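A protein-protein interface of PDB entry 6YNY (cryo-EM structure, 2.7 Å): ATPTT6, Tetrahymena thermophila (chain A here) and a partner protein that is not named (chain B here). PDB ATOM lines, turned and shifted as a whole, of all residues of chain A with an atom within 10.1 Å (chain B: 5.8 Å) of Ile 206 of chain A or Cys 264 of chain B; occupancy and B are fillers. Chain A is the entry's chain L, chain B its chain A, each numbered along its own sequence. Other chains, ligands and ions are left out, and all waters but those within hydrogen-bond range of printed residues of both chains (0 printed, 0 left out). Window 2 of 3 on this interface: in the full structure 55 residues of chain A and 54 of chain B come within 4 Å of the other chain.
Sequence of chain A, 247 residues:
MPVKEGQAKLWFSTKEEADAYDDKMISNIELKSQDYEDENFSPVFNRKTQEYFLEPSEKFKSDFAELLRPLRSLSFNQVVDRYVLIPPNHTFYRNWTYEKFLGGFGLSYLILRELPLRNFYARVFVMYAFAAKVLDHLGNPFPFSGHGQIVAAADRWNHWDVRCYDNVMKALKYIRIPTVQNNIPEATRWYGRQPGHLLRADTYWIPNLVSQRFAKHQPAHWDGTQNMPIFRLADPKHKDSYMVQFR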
ATOM      1  N   ASP A 202      14.229  15.991  -8.404  1.00  0.00           N
ATOM      2  CA  ASP A 202      14.351  17.406  -8.072  1.00  0.00           C
ATOM      3  C   ASP A 202      15.822  17.787  -8.083  1.00  0.00           C
ATOM      4  O   ASP A 202      16.590  17.333  -7.232  1.00  0.00           O
ATOM      5  CB  ASP A 202      13.724  17.695  -6.714  1.00  0.00           C
ATOM      6  CG  ASP A 202      14.020  19.089  -6.223  1.00  0.00           C
ATOM      7  OD1 ASP A 202      13.668  20.057  -6.927  1.00  0.00           O
ATOM      8  OD2 ASP A 202      14.600  19.217  -5.128  1.00  0.00           O
ATOM      9  N   THR A 203      16.207  18.615  -9.049  1.00  0.00           N
ATOM     10  CA  THR A 203      17.545  19.174  -9.121  1.00  0.00           C
ATOM     11  C   THR A 203      17.603  20.599  -8.595  1.00  0.00           C
ATOM     12  O   THR A 203      18.679  21.201  -8.581  1.00  0.00           O
ATOM     13  CB  THR A 203      18.054  19.143 -10.563  1.00  0.00           C
ATOM     14  OG1 THR A 203      17.233  19.986 -11.382  1.00  0.00           O
ATOM     15  CG2 THR A 203      18.019  17.734 -11.107  1.00  0.00           C
ATOM     16  N   TYR A 204      16.470  21.144  -8.157  1.00  0.00           N
ATOM     17  CA  TYR A 204      16.405  22.513  -7.672  1.00  0.00           C
ATOM     18  C   TYR A 204      16.799  22.635  -6.208  1.00  0.00           C
ATOM     19  O   TYR A 204      17.216  23.714  -5.779  1.00  0.00           O
ATOM     20  CB  TYR A 204      14.994  23.053  -7.885  1.00  0.00           C
ATOM     21  CG  TYR A 204      14.511  22.908  -9.306  1.00  0.00           C
ATOM     22  CD1 TYR A 204      15.262  23.390 -10.366  1.00  0.00           C
ATOM     23  CD2 TYR A 204      13.316  22.269  -9.590  1.00  0.00           C
ATOM     24  CE1 TYR A 204      14.829  23.254 -11.663  1.00  0.00           C
ATOM     25  CE2 TYR A 204      12.876  22.129 -10.885  1.00  0.00           C
ATOM     26  CZ  TYR A 204      13.637  22.623 -11.918  1.00  0.00           C
ATOM     27  OH  TYR A 204      13.205  22.485 -13.214  1.00  0.00           O
ATOM     28  N   TRP A 205      16.666  21.561  -5.439  1.00  0.00           N
ATOM     29  CA  TRP A 205      17.113  21.509  -4.055  1.00  0.00           C
ATOM     30  C   TRP A 205      18.427  20.742  -4.011  1.00  0.00           C
ATOM     31  O   TRP A 205      18.466  19.554  -4.347  1.00  0.00           O
ATOM     32  CB  TRP A 205      16.059  20.833  -3.182  1.00  0.00           C
ATOM     33  CG  TRP A 205      15.950  21.354  -1.794  1.00  0.00           C
ATOM     34  CD1 TRP A 205      15.971  22.656  -1.403  1.00  0.00           C
ATOM     35  CD2 TRP A 205      15.793  20.580  -0.605  1.00  0.00           C
ATOM     36  NE1 TRP A 205      15.835  22.741  -0.044  1.00  0.00           N
ATOM     37  CE2 TRP A 205      15.726  21.478   0.471  1.00  0.00           C
ATOM     38  CE3 TRP A 205      15.704  19.212  -0.347  1.00  0.00           C
ATOM     39  CZ2 TRP A 205      15.576  21.054   1.784  1.00  0.00           C
ATOM     40  CZ3 TRP A 205      15.556  18.794   0.954  1.00  0.00           C
ATOM     41  CH2 TRP A 205      15.492  19.710   2.004  1.00  0.00           C
ATOM     42  N   ILE A 206      19.495  21.412  -3.592  1.00  0.00           N
ATOM     43  CA  ILE A 206      20.843  20.864  -3.719  1.00  0.00           C
ATOM     44  C   ILE A 206      21.028  19.609  -2.869  1.00  0.00           C
ATOM     45  O   ILE A 206      21.860  18.764  -3.225  1.00  0.00           O
ATOM     46  CB  ILE A 206      21.908  21.922  -3.386  1.00  0.00           C
ATOM     47  CG1 ILE A 206      23.302  21.364  -3.661  1.00  0.00           C
ATOM     48  CG2 ILE A 206      21.803  22.388  -1.959  1.00  0.00           C
ATOM     49  CD1 ILE A 206      24.401  22.366  -3.499  1.00  0.00           C
ATOM     50  N   PRO A 207      20.304  19.419  -1.759  1.00  0.00           N
ATOM     51  CA  PRO A 207      20.440  18.135  -1.054  1.00  0.00           C
ATOM     52  C   PRO A 207      19.964  16.956  -1.879  1.00  0.00           C
ATOM     53  O   PRO A 207      20.577  15.883  -1.835  1.00  0.00           O
ATOM     54  CB  PRO A 207      19.593  18.338   0.207  1.00  0.00           C
ATOM     55  CG  PRO A 207      19.483  19.788   0.362  1.00  0.00           C
ATOM     56  CD  PRO A 207      19.419  20.326  -1.012  1.00  0.00           C
ATOM     57  N   ASN A 208      18.880  17.124  -2.633  1.00  0.00           N
ATOM     58  CA  ASN A 208      18.405  16.053  -3.497  1.00  0.00           C
ATOM     59  C   ASN A 208      19.264  15.916  -4.740  1.00  0.00           C
ATOM     60  O   ASN A 208      19.422  14.808  -5.262  1.00  0.00           O
ATOM     61  CB  ASN A 208      16.955  16.300  -3.889  1.00  0.00           C
ATOM     62  CG  ASN A 208      16.020  16.247  -2.710  1.00  0.00           C
ATOM     63  OD1 ASN A 208      16.302  15.594  -1.708  1.00  0.00           O
ATOM     64  ND2 ASN A 208      14.900  16.937  -2.819  1.00  0.00           N
ATOM     65  N   LEU A 209      19.821  17.025  -5.225  1.00  0.00           N
ATOM     66  CA  LEU A 209      20.732  16.960  -6.357  1.00  0.00           C
ATOM     67  C   LEU A 209      21.925  16.066  -6.055  1.00  0.00           C
ATOM     68  O   LEU A 209      22.499  15.465  -6.969  1.00  0.00           O
ATOM     69  CB  LEU A 209      21.193  18.368  -6.722  1.00  0.00           C
ATOM     70  CG  LEU A 209      22.149  18.499  -7.906  1.00  0.00           C
ATOM     71  CD1 LEU A 209      21.517  17.969  -9.170  1.00  0.00           C
ATOM     72  CD2 LEU A 209      22.556  19.943  -8.078  1.00  0.00           C
ATOM     73  N   VAL A 210      22.309  15.968  -4.787  1.00  0.00           N
ATOM     74  CA  VAL A 210      23.392  15.086  -4.369  1.00  0.00           C
ATOM     75  C   VAL A 210      22.863  13.725  -3.946  1.00  0.00           C
ATOM     76  O   VAL A 210      23.390  12.686  -4.350  1.00  0.00           O
ATOM     77  CB  VAL A 210      24.188  15.748  -3.226  1.00  0.00           C
ATOM     78  CG1 VAL A 210      25.239  14.798  -2.696  1.00  0.00           C
ATOM     79  CG2 VAL A 210      24.818  17.040  -3.692  1.00  0.00           C
ATOM     80  N   SER A 211      21.812  13.715  -3.128  1.00  0.00           N
ATOM     81  CA  SER A 211      21.312  12.464  -2.570  1.00  0.00           C
ATOM     82  C   SER A 211      20.713  11.562  -3.640  1.00  0.00           C
ATOM     83  O   SER A 211      20.900  10.342  -3.604  1.00  0.00           O
ATOM     84  CB  SER A 211      20.281  12.762  -1.485  1.00  0.00           C
ATOM     85  OG  SER A 211      19.759  11.567  -0.938  1.00  0.00           O
ATOM     86  N   GLN A 212      19.982  12.137  -4.596  1.00  0.00           N
ATOM     87  CA  GLN A 212      19.299  11.326  -5.595  1.00  0.00           C
ATOM     88  C   GLN A 212      20.251  10.688  -6.592  1.00  0.00           C
ATOM     89  O   GLN A 212      19.814   9.855  -7.392  1.00  0.00           O
ATOM     90  CB  GLN A 212      18.260  12.168  -6.329  1.00  0.00           C
ATOM     91  CG  GLN A 212      17.114  12.612  -5.448  1.00  0.00           C
ATOM     92  CD  GLN A 212      16.042  13.345  -6.212  1.00  0.00           C
ATOM     93  OE1 GLN A 212      16.276  13.849  -7.308  1.00  0.00           O
ATOM     94  NE2 GLN A 212      14.852  13.403  -5.639  1.00  0.00           N
ATOM     95  N   ARG A 213      21.531  11.057  -6.572  1.00  0.00           N
ATOM     96  CA  ARG A 213      22.521  10.381  -7.394  1.00  0.00           C
ATOM     97  C   ARG A 213      22.891   9.016  -6.841  1.00  0.00           C
ATOM     98  O   ARG A 213      23.347   8.155  -7.599  1.00  0.00           O
ATOM     99  CB  ARG A 213      23.780  11.239  -7.509  1.00  0.00           C
ATOM    100  CG  ARG A 213      23.542  12.665  -7.958  1.00  0.00           C
ATOM    101  CD  ARG A 213      23.140  12.765  -9.409  1.00  0.00           C
ATOM    102  NE  ARG A 213      21.775  12.318  -9.660  1.00  0.00           N
ATOM    103  CZ  ARG A 213      20.691  13.023  -9.361  1.00  0.00           C
ATOM    104  NH1 ARG A 213      20.805  14.209  -8.787  1.00  0.00           N
ATOM    105  NH2 ARG A 213      19.490  12.541  -9.631  1.00  0.00           N
ATOM    106  N   PHE A 214      22.707   8.802  -5.540  1.00  0.00           N
ATOM    107  CA  PHE A 214      22.990   7.527  -4.901  1.00  0.00           C
ATOM    108  C   PHE A 214      21.727   6.735  -4.605  1.00  0.00           C
ATOM    109  O   PHE A 214      21.803   5.677  -3.974  1.00  0.00           O
ATOM    110  CB  PHE A 214      23.769   7.752  -3.606  1.00  0.00           C
ATOM    111  CG  PHE A 214      25.040   8.519  -3.791  1.00  0.00           C
ATOM    112  CD1 PHE A 214      26.220   7.867  -4.090  1.00  0.00           C
ATOM    113  CD2 PHE A 214      25.058   9.894  -3.660  1.00  0.00           C
ATOM    114  CE1 PHE A 214      27.389   8.570  -4.257  1.00  0.00           C
ATOM    115  CE2 PHE A 214      26.222  10.600  -3.827  1.00  0.00           C
ATOM    116  CZ  PHE A 214      27.390   9.940  -4.126  1.00  0.00           C
ATOM    117  N   MET A 243       9.897  22.041   1.338  1.00  0.00           N
ATOM    118  CA  MET A 243      10.764  23.040   0.734  1.00  0.00           C
ATOM    119  C   MET A 243      10.117  23.736  -0.450  1.00  0.00           C
ATOM    120  O   MET A 243      10.626  24.767  -0.897  1.00  0.00           O
ATOM    121  CB  MET A 243      12.071  22.391   0.286  1.00  0.00           C
ATOM    122  CG  MET A 243      11.917  21.378  -0.836  1.00  0.00           C
ATOM    123  SD  MET A 243      10.827  20.011  -0.443  1.00  0.00           S
ATOM    124  CE  MET A 243      11.833  19.159   0.753  1.00  0.00           C
ATOM    125  N   LEU B 260      19.807  29.615  -8.128  1.00  0.00           N
ATOM    126  CA  LEU B 260      21.156  29.130  -7.869  1.00  0.00           C
ATOM    127  C   LEU B 260      21.425  27.780  -8.518  1.00  0.00           C
ATOM    128  O   LEU B 260      22.291  27.032  -8.055  1.00  0.00           O
ATOM    129  CB  LEU B 260      21.396  29.039  -6.364  1.00  0.00           C
ATOM    130  CG  LEU B 260      21.247  30.331  -5.572  1.00  0.00           C
ATOM    131  CD1 LEU B 260      21.449  30.058  -4.108  1.00  0.00           C
ATOM    132  CD2 LEU B 260      22.227  31.372  -6.050  1.00  0.00           C
ATOM    133  N   LEU B 261      20.703  27.453  -9.589  1.00  0.00           N
ATOM    134  CA  LEU B 261      20.892  26.162 -10.238  1.00  0.00           C
ATOM    135  C   LEU B 261      22.320  25.998 -10.735  1.00  0.00           C
ATOM    136  O   LEU B 261      22.995  25.015 -10.409  1.00  0.00           O
ATOM    137  CB  LEU B 261      19.909  26.009 -11.396  1.00  0.00           C
ATOM    138  CG  LEU B 261      19.861  24.616 -12.020  1.00  0.00           C
ATOM    139  CD1 LEU B 261      19.288  23.618 -11.040  1.00  0.00           C
ATOM    140  CD2 LEU B 261      19.061  24.629 -13.291  1.00  0.00           C
ATOM    141  N   LEU B 262      22.799  26.953 -11.532  1.00  0.00           N
ATOM    142  CA  LEU B 262      24.145  26.849 -12.081  1.00  0.00           C
ATOM    143  C   LEU B 262      25.195  26.852 -10.981  1.00  0.00           C
ATOM    144  O   LEU B 262      26.258  26.239 -11.135  1.00  0.00           O
ATOM    145  CB  LEU B 262      24.397  27.987 -13.066  1.00  0.00           C
ATOM    146  CG  LEU B 262      25.718  27.948 -13.833  1.00  0.00           C
ATOM    147  CD1 LEU B 262      25.795  26.728 -14.730  1.00  0.00           C
ATOM    148  CD2 LEU B 262      25.895  29.209 -14.646  1.00  0.00           C
ATOM    149  N   SER B 263      24.919  27.531  -9.869  1.00  0.00           N
ATOM    150  CA  SER B 263      25.860  27.538  -8.757  1.00  0.00           C
ATOM    151  C   SER B 263      25.845  26.219  -8.000  1.00  0.00           C
ATOM    152  O   SER B 263      26.879  25.797  -7.472  1.00  0.00           O
ATOM    153  CB  SER B 263      25.539  28.692  -7.812  1.00  0.00           C
ATOM    154  OG  SER B 263      25.473  29.911  -8.519  1.00  0.00           O
ATOM    155  N   CYS B 264      24.688  25.560  -7.928  1.00  0.00           N
ATOM    156  CA  CYS B 264      24.608  24.273  -7.252  1.00  0.00           C
ATOM    157  C   CYS B 264      25.293  23.172  -8.048  1.00  0.00           C
ATOM    158  O   CYS B 264      25.860  22.246  -7.461  1.00  0.00           O
ATOM    159  CB  CYS B 264      23.148  23.904  -6.996  1.00  0.00           C
ATOM    160  SG  CYS B 264      22.369  24.809  -5.650  1.00  0.00           S
ATOM    161  N   TYR B 265      25.242  23.244  -9.376  1.00  0.00           N
ATOM    162  CA  TYR B 265      25.956  22.273 -10.194  1.00  0.00           C
ATOM    163  C   TYR B 265      27.453  22.547 -10.205  1.00  0.00           C
ATOM    164  O   TYR B 265      28.258  21.610 -10.174  1.00  0.00           O
ATOM    165  CB  TYR B 265      25.419  22.293 -11.622  1.00  0.00           C
ATOM    166  CG  TYR B 265      24.158  21.500 -11.847  1.00  0.00           C
ATOM    167  CD1 TYR B 265      24.212  20.209 -12.339  1.00  0.00           C
ATOM    168  CD2 TYR B 265      22.914  22.046 -11.587  1.00  0.00           C
ATOM    169  CE1 TYR B 265      23.069  19.483 -12.558  1.00  0.00           C
ATOM    170  CE2 TYR B 265      21.764  21.324 -11.803  1.00  0.00           C
ATOM    171  CZ  TYR B 265      21.848  20.045 -12.287  1.00  0.00           C
ATOM    172  OH  TYR B 265      20.706  19.318 -12.508  1.00  0.00           O
ATOM    173  N   SER B 266      27.842  23.821 -10.250  1.00  0.00           N
ATOM    174  CA  SER B 266      29.254  24.165 -10.341  1.00  0.00           C
ATOM    175  C   SER B 266      30.025  23.739  -9.100  1.00  0.00           C
ATOM    176  O   SER B 266      31.197  23.363  -9.199  1.00  0.00           O
ATOM    177  CB  SER B 266      29.409  25.665 -10.565  1.00  0.00           C
ATOM    178  OG  SER B 266      28.745  26.074 -11.742  1.00  0.00           O
ATOM    179  N   ILE B 267      29.395  23.799  -7.926  1.00  0.00           N
ATOM    180  CA  ILE B 267      30.078  23.381  -6.708  1.00  0.00           C
ATOM    181  C   ILE B 267      30.353  21.885  -6.742  1.00  0.00           C
ATOM    182  O   ILE B 267      31.372  21.420  -6.218  1.00  0.00           O
ATOM    183  CB  ILE B 267      29.256  23.786  -5.469  1.00  0.00           C
ATOM    184  CG1 ILE B 267      29.978  23.400  -4.183  1.00  0.00           C
ATOM    185  CG2 ILE B 267      27.893  23.138  -5.487  1.00  0.00           C
ATOM    186  CD1 ILE B 267      31.252  24.144  -3.968  1.00  0.00           C
ATOM    187  N   ILE B 268      29.461  21.111  -7.357  1.00  0.00           N
ATOM    188  CA  ILE B 268      29.699  19.682  -7.522  1.00  0.00           C
ATOM    189  C   ILE B 268      30.773  19.447  -8.573  1.00  0.00           C
ATOM    190  O   ILE B 268      31.694  18.647  -8.379  1.00  0.00           O
ATOM    191  CB  ILE B 268      28.385  18.969  -7.885  1.00  0.00           C
ATOM    192  CG1 ILE B 268      27.336  19.223  -6.802  1.00  0.00           C
ATOM    193  CG2 ILE B 268      28.616  17.485  -8.072  1.00  0.00           C
ATOM    194  CD1 ILE B 268      25.982  18.659  -7.112  1.00  0.00           C
ATOM    195  N   ILE B 269      30.668  20.145  -9.704  1.00  0.00           N
ATOM    196  CA  ILE B 269      31.710  20.090 -10.724  1.00  0.00           C
ATOM    197  C   ILE B 269      33.058  20.444 -10.113  1.00  0.00           C
ATOM    198  O   ILE B 269      34.051  19.728 -10.282  1.00  0.00           O
ATOM    199  CB  ILE B 269      31.356  21.034 -11.886  1.00  0.00           C
ATOM    200  CG1 ILE B 269      30.094  20.551 -12.595  1.00  0.00           C
ATOM    201  CG2 ILE B 269      32.499  21.139 -12.861  1.00  0.00           C
ATOM    202  CD1 ILE B 269      29.479  21.584 -13.489  1.00  0.00           C
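SG of Cys 264 of chain B sits at hydrogen-bond distance from O of Leu 260 of chain B (3.3 Å). The backbone carbonyl oxygen (O) of Leu 209 of chain A sits at hydrogen-bond distance from the guanidinium group (NH1) of Arg 213 of chain A (2.8 Å).
Among the printed residues, merely in contact across the chains: Thr 203 of chain A with Leu 261 of chain B (3.5 Å), Thr 203 of chain A with Tyr 265 of chain B (3.3 Å), Ile 206 of chain A with Cys 264 of chain B (3.7 Å), Leu 209 of chain A with Tyr 265 of chain B (3.7 Å), Leu 209 of chain A with Ile 268 of chain B (3.8 Å) and Val 210 of chain A with Ile 268 of chain B (3.96 Å).
Ile 206 of chain A touches one residue of chain B. Printed residues of chain B within 4 Å of Leu 209 of chain A: Tyr 265 (3.7 Å) and Ile 268 (3.8 Å). Of the printed residues of chain B, Val 210 of chain A touches Ile 268. No residue of chain A comes within 4 Å of Ser 263 of chain B. Printed residues of chain A within 4 Å of Cys 264 of chain B: Ile 206. No residue of chain A comes within 4 Å of Ser 266 of chain B. Of the printed residues of chain A, Ile 268 of chain B touches Leu 209 and Val 210.
Hydrophobic or aromatic side chains of chain B that line the printed part of chain A: Leu 261, Tyr 265 and Ile 268. Hydrophobic or aromatic side chains of chain A within 4 Å of the printed part of chain B: Ile 206, Leu 209 and Val 210. Among the printed residues, no Asp or Glu carboxylate lies within 4 Å of a Lys or Arg side-chain nitrogen of the other chain.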
